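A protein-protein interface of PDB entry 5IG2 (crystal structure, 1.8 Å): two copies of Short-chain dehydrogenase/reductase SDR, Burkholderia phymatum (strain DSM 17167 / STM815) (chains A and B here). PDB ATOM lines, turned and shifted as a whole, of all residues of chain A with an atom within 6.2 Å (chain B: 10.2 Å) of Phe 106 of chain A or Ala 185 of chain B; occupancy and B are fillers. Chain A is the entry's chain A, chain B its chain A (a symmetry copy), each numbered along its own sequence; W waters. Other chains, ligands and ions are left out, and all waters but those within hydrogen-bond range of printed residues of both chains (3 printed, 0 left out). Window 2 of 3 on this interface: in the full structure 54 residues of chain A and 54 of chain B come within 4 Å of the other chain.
The side-chain carboxylate (OD2) of Asp 181 of chain B is in hydrogen-bond range of the backbone NH (N) of Leu 107 of chain A (2.9 Å).
N of Ser 160 of chain A sits at hydrogen-bond distance from OD1 of Asp 181 of chain B.
The backbone carbonyl oxygen of Ser 160 of chain A is in hydrogen-bond range of the backbone NH of Gly 105 of chain A (2.8 Å).
The backbone NH of Phe 106 of chain A is in hydrogen-bond range of the side-chain hydroxyl of Ser 223 of chain A (3.0 Å).
Among the printed residues, pairs that only touch across the chains: Phe 106 of chain A with Asp 181 of chain B, Phe 106 of chain A with Ala 185 of chain B, Leu 107 of chain A with Leu 174 of chain B, Trp 108 of chain A with Val 130 of chain B, Trp 108 of chain A with Arg 131 of chain B, Trp 108 of chain A with Ala 134 of chain B, Trp 108 of chain A with Leu 138 of chain B, Trp 108 of chain A with Leu 178 of chain B, Trp 108 of chain A with Asp 181 of chain B, Trp 108 of chain A with Leu 182 of chain B, Trp 108 of chain A with Ala 185 of chain B, Ser 110 of chain A with Arg 131 of chain B and Ser 160 of chain A with Thr 177 of chain B.
Phe 106 of chain A touches two residues of chain B.
Ala 185 of chain B touches just these residues of chain A: Phe 106 (3.9 Å) and Trp 108 (3.7 Å).
No residue of chain B comes within 4 Å of Gly 105 of chain A.
Of the printed residues of chain B, Ser 160 of chain A touches Thr 177 (3.7 Å) and Asp 181 (2.8 Å).
No residue of chain B comes within 4 Å of Ser 223 of chain A.
Printed residues of chain A within 4 Å of Ala 134 of chain B: Trp 108.
Printed residues of chain A within 4 Å of Thr 177 of chain B: Ser 160 (3.7 Å).
Asn 184 of chain B touches none of the printed residues of chain A.
Gly 139 of chain B touches none of the printed residues of chain A.
Printed residues of chain B that touch a printed residue of chain A: Val 130, Arg 131, Ala 134, Leu 138, Leu 174, Thr 177, Leu 178, Asp 181, Leu 182 and Ala 185.
Hydrophobic or aromatic side chains of chain B within 4 Å of the printed part of chain A: Ala 134, Leu 138, Leu 174, Leu 178, Leu 182 and Ala 185.
Hydrophobic or aromatic side chains of chain A that line the printed part of chain B: Phe 106, Leu 107 and Trp 108.
Along chain A the printed residues that touch a printed residue of chain B span positions 106 to 160.
Among the printed residues, 15 pairs touch across the chains.
Among the printed residues, no Asp or Glu carboxylate lies within 4 Å of a Lys or Arg side-chain nitrogen of the other chain.
No position is printed for both chains.
Water W3 lies within hydrogen-bond range of the backbone carbonyl oxygen (O) of Trp 108 of chain A (2.5 Å) and the backbone carbonyl oxygen (O) of Arg 131 of chain B (3.5 Å).
Water W2 lies within hydrogen-bond range of OD1 of Asp 181 of chain B, OG of Ser 160 of chain A and ND2 of Asn 184 of chain B.
Water W1 bridges OD2 of Asp 181 of chain B (2.7 Å) and O of Gly 105 of chain A (2.9 Å).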
ATOM      1  N   GLY A 104     -21.598  -0.815  -2.345  1.00  0.00           N
ATOM      2  CA  GLY A 104     -22.022   0.501  -2.782  1.00  0.00           C
ATOM      3  C   GLY A 104     -20.855   1.441  -3.033  1.00  0.00           C
ATOM      4  O   GLY A 104     -19.689   1.073  -2.884  1.00  0.00           O
ATOM      5  N   GLY A 105     -21.201   2.673  -3.417  1.00  0.00           N
ATOM      6  CA  GLY A 105     -20.231   3.695  -3.771  1.00  0.00           C
ATOM      7  C   GLY A 105     -20.359   4.133  -5.222  1.00  0.00           C
ATOM      8  O   GLY A 105     -20.990   3.434  -6.025  1.00  0.00           O
ATOM      9  N   PHE A 106     -19.786   5.291  -5.568  1.00  0.00           N
ATOM     10  CA  PHE A 106     -19.683   5.696  -6.971  1.00  0.00           C
ATOM     11  C   PHE A 106     -19.201   4.520  -7.815  1.00  0.00           C
ATOM     12  O   PHE A 106     -18.257   3.818  -7.437  1.00  0.00           O
ATOM     13  CB  PHE A 106     -18.713   6.876  -7.123  1.00  0.00           C
ATOM     14  CG  PHE A 106     -19.197   8.174  -6.512  1.00  0.00           C
ATOM     15  CD1 PHE A 106     -20.538   8.381  -6.221  1.00  0.00           C
ATOM     16  CD2 PHE A 106     -18.297   9.198  -6.255  1.00  0.00           C
ATOM     17  CE1 PHE A 106     -20.969   9.578  -5.667  1.00  0.00           C
ATOM     18  CE2 PHE A 106     -18.722  10.405  -5.703  1.00  0.00           C
ATOM     19  CZ  PHE A 106     -20.059  10.595  -5.413  1.00  0.00           C
ATOM     20  N   LEU A 107     -19.855   4.309  -8.964  1.00  0.00           N
ATOM     21  CA  LEU A 107     -19.727   3.027  -9.657  1.00  0.00           C
ATOM     22  C   LEU A 107     -18.277   2.708 -10.014  1.00  0.00           C
ATOM     23  O   LEU A 107     -17.827   1.567  -9.844  1.00  0.00           O
ATOM     24  CB  LEU A 107     -20.607   3.011 -10.909  1.00  0.00           C
ATOM     25  CG  LEU A 107     -20.647   1.644 -11.597  1.00  0.00           C
ATOM     26  CD1 LEU A 107     -21.234   0.591 -10.652  1.00  0.00           C
ATOM     27  CD2 LEU A 107     -21.439   1.718 -12.893  1.00  0.00           C
ATOM     28  N   TRP A 108     -17.526   3.703 -10.500  1.00  0.00           N
ATOM     29  CA  TRP A 108     -16.157   3.473 -10.958  1.00  0.00           C
ATOM     30  C   TRP A 108     -15.180   3.271  -9.808  1.00  0.00           C
ATOM     31  O   TRP A 108     -14.054   2.825 -10.049  1.00  0.00           O
ATOM     32  CB  TRP A 108     -15.692   4.646 -11.841  1.00  0.00           C
ATOM     33  CG  TRP A 108     -15.723   5.953 -11.104  1.00  0.00           C
ATOM     34  CD1 TRP A 108     -14.720   6.493 -10.361  1.00  0.00           C
ATOM     35  CD2 TRP A 108     -16.836   6.847 -10.990  1.00  0.00           C
ATOM     36  NE1 TRP A 108     -15.131   7.681  -9.808  1.00  0.00           N
ATOM     37  CE2 TRP A 108     -16.429   7.919 -10.176  1.00  0.00           C
ATOM     38  CE3 TRP A 108     -18.138   6.848 -11.504  1.00  0.00           C
ATOM     39  CZ2 TRP A 108     -17.270   8.987  -9.864  1.00  0.00           C
ATOM     40  CZ3 TRP A 108     -18.975   7.909 -11.192  1.00  0.00           C
ATOM     41  CH2 TRP A 108     -18.540   8.961 -10.377  1.00  0.00           C
ATOM     42  N   GLU A 109     -15.569   3.586  -8.569  1.00  0.00           N
ATOM     43  CA  GLU A 109     -14.658   3.402  -7.449  1.00  0.00           C
ATOM     44  C   GLU A 109     -14.637   1.969  -6.940  1.00  0.00           C
ATOM     45  O   GLU A 109     -13.705   1.593  -6.219  1.00  0.00           O
ATOM     46  CB  GLU A 109     -15.027   4.354  -6.309  1.00  0.00           C
ATOM     47  CG  GLU A 109     -14.865   5.828  -6.683  1.00  0.00           C
ATOM     48  CD  GLU A 109     -15.155   6.760  -5.521  1.00  0.00           C
ATOM     49  OE1 GLU A 109     -15.863   6.324  -4.582  1.00  0.00           O
ATOM     50  OE2 GLU A 109     -14.670   7.917  -5.551  1.00  0.00           O
ATOM     51  N   SER A 110     -15.644   1.172  -7.289  1.00  0.00           N
ATOM     52  CA  SER A 110     -15.698  -0.226  -6.887  1.00  0.00           C
ATOM     53  C   SER A 110     -14.619  -1.033  -7.600  1.00  0.00           C
ATOM     54  O   SER A 110     -14.211  -0.718  -8.720  1.00  0.00           O
ATOM     55  CB  SER A 110     -17.075  -0.809  -7.202  1.00  0.00           C
ATOM     56  OG  SER A 110     -18.089  -0.145  -6.464  1.00  0.00           O
ATOM     57  N   SER A 160     -25.249   5.262  -6.330  1.00  0.00           N
ATOM     58  CA  SER A 160     -24.217   4.679  -5.471  1.00  0.00           C
ATOM     59  C   SER A 160     -24.482   3.221  -5.105  1.00  0.00           C
ATOM     60  O   SER A 160     -23.879   2.706  -4.157  1.00  0.00           O
ATOM     61  CB  SER A 160     -24.023   5.502  -4.188  1.00  0.00           C
ATOM     62  OG  SER A 160     -23.324   6.701  -4.443  1.00  0.00           O
ATOM     63  N   THR A 221     -13.643   4.281   0.045  1.00  0.00           N
ATOM     64  CA  THR A 221     -13.636   5.673  -0.357  1.00  0.00           C
ATOM     65  C   THR A 221     -14.740   6.436   0.373  1.00  0.00           C
ATOM     66  O   THR A 221     -15.587   5.855   1.059  1.00  0.00           O
ATOM     67  CB  THR A 221     -13.839   5.801  -1.864  1.00  0.00           C
ATOM     68  OG1 THR A 221     -15.152   5.337  -2.195  1.00  0.00           O
ATOM     69  CG2 THR A 221     -12.806   4.979  -2.622  1.00  0.00           C
ATOM     70  N   SER A 223     -17.341   7.955  -0.923  1.00  0.00           N
ATOM     71  CA  SER A 223     -18.678   7.605  -1.403  1.00  0.00           C
ATOM     72  C   SER A 223     -19.084   6.202  -0.963  1.00  0.00           C
ATOM     73  O   SER A 223     -20.277   5.937  -0.764  1.00  0.00           O
ATOM     74  CB  SER A 223     -18.745   7.715  -2.930  1.00  0.00           C
ATOM     75  OG  SER A 223     -18.076   6.632  -3.554  1.00  0.00           O
ATOM     76  N   GLN A 224     -18.118   5.293  -0.834  1.00  0.00           N
ATOM     77  CA  GLN A 224     -18.430   3.952  -0.371  1.00  0.00           C
ATOM     78  C   GLN A 224     -18.843   3.971   1.093  1.00  0.00           C
ATOM     79  O   GLN A 224     -19.793   3.281   1.482  1.00  0.00           O
ATOM     80  CB  GLN A 224     -17.232   3.032  -0.597  1.00  0.00           C
ATOM     81  CG  GLN A 224     -16.947   2.793  -2.076  1.00  0.00           C
ATOM     82  CD  GLN A 224     -15.622   2.111  -2.326  1.00  0.00           C
ATOM     83  OE1 GLN A 224     -14.766   2.049  -1.448  1.00  0.00           O
ATOM     84  NE2 GLN A 224     -15.448   1.593  -3.531  1.00  0.00           N
ATOM     85  N   ALA A 227     -22.365   5.377   1.170  1.00  0.00           N
ATOM     86  CA  ALA A 227     -23.374   4.423   0.716  1.00  0.00           C
ATOM     87  C   ALA A 227     -23.633   3.356   1.774  1.00  0.00           C
ATOM     88  O   ALA A 227     -24.780   2.932   1.974  1.00  0.00           O
ATOM     89  CB  ALA A 227     -22.941   3.774  -0.600  1.00  0.00           C
ATOM     90  N   ALA B 127     -18.266  -3.166 -17.010  1.00  0.00           N
ATOM     91  CA  ALA B 127     -17.780  -2.806 -15.680  1.00  0.00           C
ATOM     92  C   ALA B 127     -16.294  -2.438 -15.701  1.00  0.00           C
ATOM     93  O   ALA B 127     -15.884  -1.427 -15.119  1.00  0.00           O
ATOM     94  CB  ALA B 127     -18.033  -3.964 -14.712  1.00  0.00           C
ATOM     95  N   VAL B 130     -15.770   1.022 -17.417  1.00  0.00           N
ATOM     96  CA  VAL B 130     -16.136   2.122 -16.528  1.00  0.00           C
ATOM     97  C   VAL B 130     -15.092   2.276 -15.434  1.00  0.00           C
ATOM     98  O   VAL B 130     -14.601   3.382 -15.170  1.00  0.00           O
ATOM     99  CB  VAL B 130     -17.546   1.891 -15.948  1.00  0.00           C
ATOM    100  CG1 VAL B 130     -17.857   2.885 -14.836  1.00  0.00           C
ATOM    101  CG2 VAL B 130     -18.573   1.984 -17.061  1.00  0.00           C
ATOM    102  N   ARG B 131     -14.712   1.161 -14.804  1.00  0.00           N
ATOM    103  CA  ARG B 131     -13.781   1.227 -13.679  1.00  0.00           C
ATOM    104  C   ARG B 131     -12.436   1.793 -14.104  1.00  0.00           C
ATOM    105  O   ARG B 131     -11.829   2.588 -13.378  1.00  0.00           O
ATOM    106  CB  ARG B 131     -13.593  -0.162 -13.069  1.00  0.00           C
ATOM    107  CG  ARG B 131     -12.563  -0.199 -11.932  1.00  0.00           C
ATOM    108  CD  ARG B 131     -12.452  -1.604 -11.335  1.00  0.00           C
ATOM    109  NE  ARG B 131     -12.139  -2.594 -12.362  1.00  0.00           N
ATOM    110  CZ  ARG B 131     -10.928  -2.790 -12.873  1.00  0.00           C
ATOM    111  NH1 ARG B 131      -9.895  -2.072 -12.450  1.00  0.00           N
ATOM    112  NH2 ARG B 131     -10.752  -3.713 -13.810  1.00  0.00           N
ATOM    113  N   ALA B 134     -13.264   5.751 -16.377  1.00  0.00           N
ATOM    114  CA  ALA B 134     -13.898   6.900 -15.734  1.00  0.00           C
ATOM    115  C   ALA B 134     -12.923   7.701 -14.881  1.00  0.00           C
ATOM    116  O   ALA B 134     -12.944   8.942 -14.982  1.00  0.00           O
ATOM    117  CB  ALA B 134     -15.118   6.473 -14.904  1.00  0.00           C
ATOM    118  N   PRO B 135     -12.052   7.092 -14.057  1.00  0.00           N
ATOM    119  CA  PRO B 135     -11.066   7.910 -13.328  1.00  0.00           C
ATOM    120  C   PRO B 135     -10.157   8.694 -14.258  1.00  0.00           C
ATOM    121  O   PRO B 135      -9.867   9.868 -13.994  1.00  0.00           O
ATOM    122  CB  PRO B 135     -10.282   6.875 -12.506  1.00  0.00           C
ATOM    123  CG  PRO B 135     -11.159   5.708 -12.421  1.00  0.00           C
ATOM    124  CD  PRO B 135     -11.946   5.671 -13.696  1.00  0.00           C
ATOM    125  N   LEU B 138     -12.247  11.571 -15.459  1.00  0.00           N
ATOM    126  CA  LEU B 138     -12.474  12.552 -14.407  1.00  0.00           C
ATOM    127  C   LEU B 138     -11.216  13.351 -14.111  1.00  0.00           C
ATOM    128  O   LEU B 138     -11.301  14.534 -13.769  1.00  0.00           O
ATOM    129  CB  LEU B 138     -12.981  11.865 -13.140  1.00  0.00           C
ATOM    130  CG  LEU B 138     -14.401  11.312 -13.258  1.00  0.00           C
ATOM    131  CD1 LEU B 138     -14.699  10.284 -12.161  1.00  0.00           C
ATOM    132  CD2 LEU B 138     -15.408  12.452 -13.219  1.00  0.00           C
ATOM    133  N   GLY B 139     -10.043  12.737 -14.252  1.00  0.00           N
ATOM    134  CA  GLY B 139      -8.810  13.451 -13.976  1.00  0.00           C
ATOM    135  C   GLY B 139      -8.388  14.446 -15.044  1.00  0.00           C
ATOM    136  O   GLY B 139      -7.547  15.308 -14.768  1.00  0.00           O
ATOM    137  N   ASN B 141     -10.151  16.827 -16.537  1.00  0.00           N
ATOM    138  CA  ASN B 141     -10.826  18.127 -16.457  1.00  0.00           C
ATOM    139  C   ASN B 141     -11.184  18.646 -17.851  1.00  0.00           C
ATOM    140  O   ASN B 141     -10.956  19.813 -18.189  1.00  0.00           O
ATOM    141  CB  ASN B 141      -9.986  19.143 -15.682  1.00  0.00           C
ATOM    142  CG  ASN B 141      -9.655  18.664 -14.279  1.00  0.00           C
ATOM    143  OD1 ASN B 141     -10.488  18.051 -13.603  1.00  0.00           O
ATOM    144  ND2 ASN B 141      -8.427  18.930 -13.838  1.00  0.00           N
ATOM    145  N   LEU B 174     -26.766  -0.468 -14.497  1.00  0.00           N
ATOM    146  CA  LEU B 174     -25.486   0.100 -14.081  1.00  0.00           C
ATOM    147  C   LEU B 174     -25.234   1.425 -14.784  1.00  0.00           C
ATOM    148  O   LEU B 174     -24.644   2.332 -14.189  1.00  0.00           O
ATOM    149  CB  LEU B 174     -24.335  -0.882 -14.327  1.00  0.00           C
ATOM    150  CG  LEU B 174     -23.741  -1.063 -15.725  1.00  0.00           C
ATOM    151  CD1 LEU B 174     -22.675  -0.001 -16.068  1.00  0.00           C
ATOM    152  CD2 LEU B 174     -23.155  -2.473 -15.837  1.00  0.00           C
ATOM    153  N   THR B 177     -27.355   4.089 -13.146  1.00  0.00           N
ATOM    154  CA  THR B 177     -26.725   4.479 -11.888  1.00  0.00           C
ATOM    155  C   THR B 177     -25.499   5.343 -12.143  1.00  0.00           C
ATOM    156  O   THR B 177     -25.267   6.333 -11.434  1.00  0.00           O
ATOM    157  CB  THR B 177     -26.329   3.250 -11.071  1.00  0.00           C
ATOM    158  OG1 THR B 177     -27.452   2.357 -10.957  1.00  0.00           O
ATOM    159  CG2 THR B 177     -25.882   3.689  -9.668  1.00  0.00           C
ATOM    160  N   LEU B 178     -24.701   4.968 -13.150  1.00  0.00           N
ATOM    161  CA  LEU B 178     -23.531   5.747 -13.542  1.00  0.00           C
ATOM    162  C   LEU B 178     -23.900   7.191 -13.846  1.00  0.00           C
ATOM    163  O   LEU B 178     -23.185   8.127 -13.462  1.00  0.00           O
ATOM    164  CB  LEU B 178     -22.880   5.095 -14.766  1.00  0.00           C
ATOM    165  CG  LEU B 178     -21.637   5.814 -15.302  1.00  0.00           C
ATOM    166  CD1 LEU B 178     -20.563   5.953 -14.221  1.00  0.00           C
ATOM    167  CD2 LEU B 178     -21.088   5.096 -16.543  1.00  0.00           C
ATOM    168  N   TYR B 179     -25.021   7.384 -14.541  1.00  0.00           N
ATOM    169  CA  TYR B 179     -25.486   8.724 -14.867  1.00  0.00           C
ATOM    170  C   TYR B 179     -25.670   9.557 -13.606  1.00  0.00           C
ATOM    171  O   TYR B 179     -25.248  10.717 -13.548  1.00  0.00           O
ATOM    172  CB  TYR B 179     -26.790   8.626 -15.662  1.00  0.00           C
ATOM    173  CG  TYR B 179     -27.457   9.959 -15.887  1.00  0.00           C
ATOM    174  CD1 TYR B 179     -27.100  10.757 -16.962  1.00  0.00           C
ATOM    175  CD2 TYR B 179     -28.447  10.425 -15.015  1.00  0.00           C
ATOM    176  CE1 TYR B 179     -27.716  11.998 -17.170  1.00  0.00           C
ATOM    177  CE2 TYR B 179     -29.067  11.659 -15.212  1.00  0.00           C
ATOM    178  CZ  TYR B 179     -28.695  12.439 -16.293  1.00  0.00           C
ATOM    179  OH  TYR B 179     -29.303  13.658 -16.498  1.00  0.00           O
ATOM    180  N   HIS B 180     -26.297   8.973 -12.582  1.00  0.00           N
ATOM    181  CA  HIS B 180     -26.491   9.686 -11.322  1.00  0.00           C
ATOM    182  C   HIS B 180     -25.178   9.867 -10.572  1.00  0.00           C
ATOM    183  O   HIS B 180     -24.931  10.935 -10.003  1.00  0.00           O
ATOM    184  CB  HIS B 180     -27.498   8.947 -10.437  1.00  0.00           C
ATOM    185  CG  HIS B 180     -28.883   8.872 -11.005  1.00  0.00           C
ATOM    186  ND1 HIS B 180     -29.627   9.992 -11.317  1.00  0.00           N
ATOM    187  CD2 HIS B 180     -29.674   7.807 -11.286  1.00  0.00           C
ATOM    188  CE1 HIS B 180     -30.807   9.620 -11.780  1.00  0.00           C
ATOM    189  NE2 HIS B 180     -30.864   8.300 -11.767  1.00  0.00           N
ATOM    190  N   ASP B 181     -24.331   8.830 -10.539  1.00  0.00           N
ATOM    191  CA  ASP B 181     -23.057   8.939  -9.825  1.00  0.00           C
ATOM    192  C   ASP B 181     -22.167  10.021 -10.430  1.00  0.00           C
ATOM    193  O   ASP B 181     -21.496  10.759  -9.702  1.00  0.00           O
ATOM    194  CB  ASP B 181     -22.308   7.601  -9.835  1.00  0.00           C
ATOM    195  CG  ASP B 181     -23.020   6.513  -9.064  1.00  0.00           C
ATOM    196  OD1 ASP B 181     -23.976   6.798  -8.326  1.00  0.00           O
ATOM    197  OD2 ASP B 181     -22.594   5.357  -9.192  1.00  0.00           O
ATOM    198  N   LEU B 182     -22.121  10.109 -11.765  1.00  0.00           N
ATOM    199  CA  LEU B 182     -21.295  11.136 -12.391  1.00  0.00           C
ATOM    200  C   LEU B 182     -21.788  12.531 -12.023  1.00  0.00           C
ATOM    201  O   LEU B 182     -20.987  13.451 -11.811  1.00  0.00           O
ATOM    202  CB  LEU B 182     -21.278  10.944 -13.906  1.00  0.00           C
ATOM    203  CG  LEU B 182     -20.447   9.748 -14.395  1.00  0.00           C
ATOM    204  CD1 LEU B 182     -20.652   9.503 -15.883  1.00  0.00           C
ATOM    205  CD2 LEU B 182     -18.955   9.952 -14.100  1.00  0.00           C
ATOM    206  N   ARG B 183     -23.106  12.703 -11.922  1.00  0.00           N
ATOM    207  CA  ARG B 183     -23.646  14.003 -11.548  1.00  0.00           C
ATOM    208  C   ARG B 183     -23.343  14.313 -10.091  1.00  0.00           C
ATOM    209  O   ARG B 183     -22.885  15.413  -9.763  1.00  0.00           O
ATOM    210  CB  ARG B 183     -25.147  14.039 -11.832  1.00  0.00           C
ATOM    211  CG  ARG B 183     -25.434  14.134 -13.333  1.00  0.00           C
ATOM    212  CD  ARG B 183     -26.871  13.792 -13.700  1.00  0.00           C
ATOM    213  NE  ARG B 183     -27.837  14.780 -13.227  1.00  0.00           N
ATOM    214  CZ  ARG B 183     -28.081  15.939 -13.833  1.00  0.00           C
ATOM    215  NH1 ARG B 183     -27.415  16.276 -14.935  1.00  0.00           N
ATOM    216  NH2 ARG B 183     -28.985  16.764 -13.328  1.00  0.00           N
ATOM    217  N   ASN B 184     -23.568  13.344  -9.203  1.00  0.00           N
ATOM    218  CA  ASN B 184     -23.248  13.564  -7.797  1.00  0.00           C
ATOM    219  C   ASN B 184     -21.763  13.834  -7.606  1.00  0.00           C
ATOM    220  O   ASN B 184     -21.379  14.619  -6.735  1.00  0.00           O
ATOM    221  CB  ASN B 184     -23.699  12.363  -6.964  1.00  0.00           C
ATOM    222  CG  ASN B 184     -25.200  12.302  -6.808  1.00  0.00           C
ATOM    223  OD1 ASN B 184     -25.882  13.313  -6.943  1.00  0.00           O
ATOM    224  ND2 ASN B 184     -25.726  11.120  -6.526  1.00  0.00           N
ATOM    225  N   ALA B 185     -20.914  13.218  -8.427  1.00  0.00           N
ATOM    226  CA  ALA B 185     -19.486  13.455  -8.301  1.00  0.00           C
ATOM    227  C   ALA B 185     -19.101  14.831  -8.829  1.00  0.00           C
ATOM    228  O   ALA B 185     -18.124  15.422  -8.355  1.00  0.00           O
ATOM    229  CB  ALA B 185     -18.714  12.363  -9.036  1.00  0.00           C
ATOM    230  N   GLY B 186     -19.866  15.359  -9.785  1.00  0.00           N
ATOM    231  CA  GLY B 186     -19.516  16.587 -10.467  1.00  0.00           C
ATOM    232  C   GLY B 186     -18.503  16.341 -11.572  1.00  0.00           C
ATOM    233  O   GLY B 186     -17.879  15.284 -11.668  1.00  0.00           O
ATOM    234  N   GLY B 187     -18.337  17.343 -12.425  1.00  0.00           N
ATOM    235  CA  GLY B 187     -17.376  17.269 -13.508  1.00  0.00           C
ATOM    236  C   GLY B 187     -18.047  17.193 -14.871  1.00  0.00           C
ATOM    237  O   GLY B 187     -19.271  17.240 -15.007  1.00  0.00           O
ATOM    238  N   GLU B 188     -17.203  17.056 -15.893  1.00  0.00           N
ATOM    239  CA  GLU B 188     -17.631  17.141 -17.282  1.00  0.00           C
ATOM    240  C   GLU B 188     -17.740  15.780 -17.960  1.00  0.00           C
ATOM    241  O   GLU B 188     -17.802  15.709 -19.194  1.00  0.00           O
ATOM    242  CB  GLU B 188     -16.674  18.036 -18.061  1.00  0.00           C
ATOM    243  CG  GLU B 188     -16.651  19.456 -17.562  1.00  0.00           C
ATOM    244  CD  GLU B 188     -15.630  20.278 -18.301  1.00  0.00           C
ATOM    245  OE1 GLU B 188     -14.510  20.447 -17.769  1.00  0.00           O
ATOM    246  OE2 GLU B 188     -15.941  20.727 -19.427  1.00  0.00           O
ATOM    247  N   VAL B 189     -17.755  14.704 -17.189  1.00  0.00           N
ATOM    248  CA  VAL B 189     -17.878  13.357 -17.725  1.00  0.00           C
ATOM    249  C   VAL B 189     -19.339  12.952 -17.656  1.00  0.00           C
ATOM    250  O   VAL B 189     -19.960  13.039 -16.590  1.00  0.00           O
ATOM    251  CB  VAL B 189     -16.995  12.371 -16.944  1.00  0.00           C
ATOM    252  CG1 VAL B 189     -17.101  10.980 -17.552  1.00  0.00           C
ATOM    253  CG2 VAL B 189     -15.550  12.875 -16.923  1.00  0.00           C
ATOM    254  N   GLY B 190     -19.893  12.525 -18.792  1.00  0.00           N
ATOM    255  CA  GLY B 190     -21.260  12.058 -18.876  1.00  0.00           C
ATOM    256  C   GLY B 190     -21.315  10.653 -19.457  1.00  0.00           C
ATOM    257  O   GLY B 190     -20.284  10.039 -19.752  1.00  0.00           O
HETATM  258  O   HOH W   1     -22.972   2.921  -8.046  1.00  0.00           O
HETATM  259  O   HOH W   2     -24.137   8.670  -6.414  1.00  0.00           O
HETATM  260  O   HOH W   3     -11.545   3.235  -9.961  1.00  0.00           O
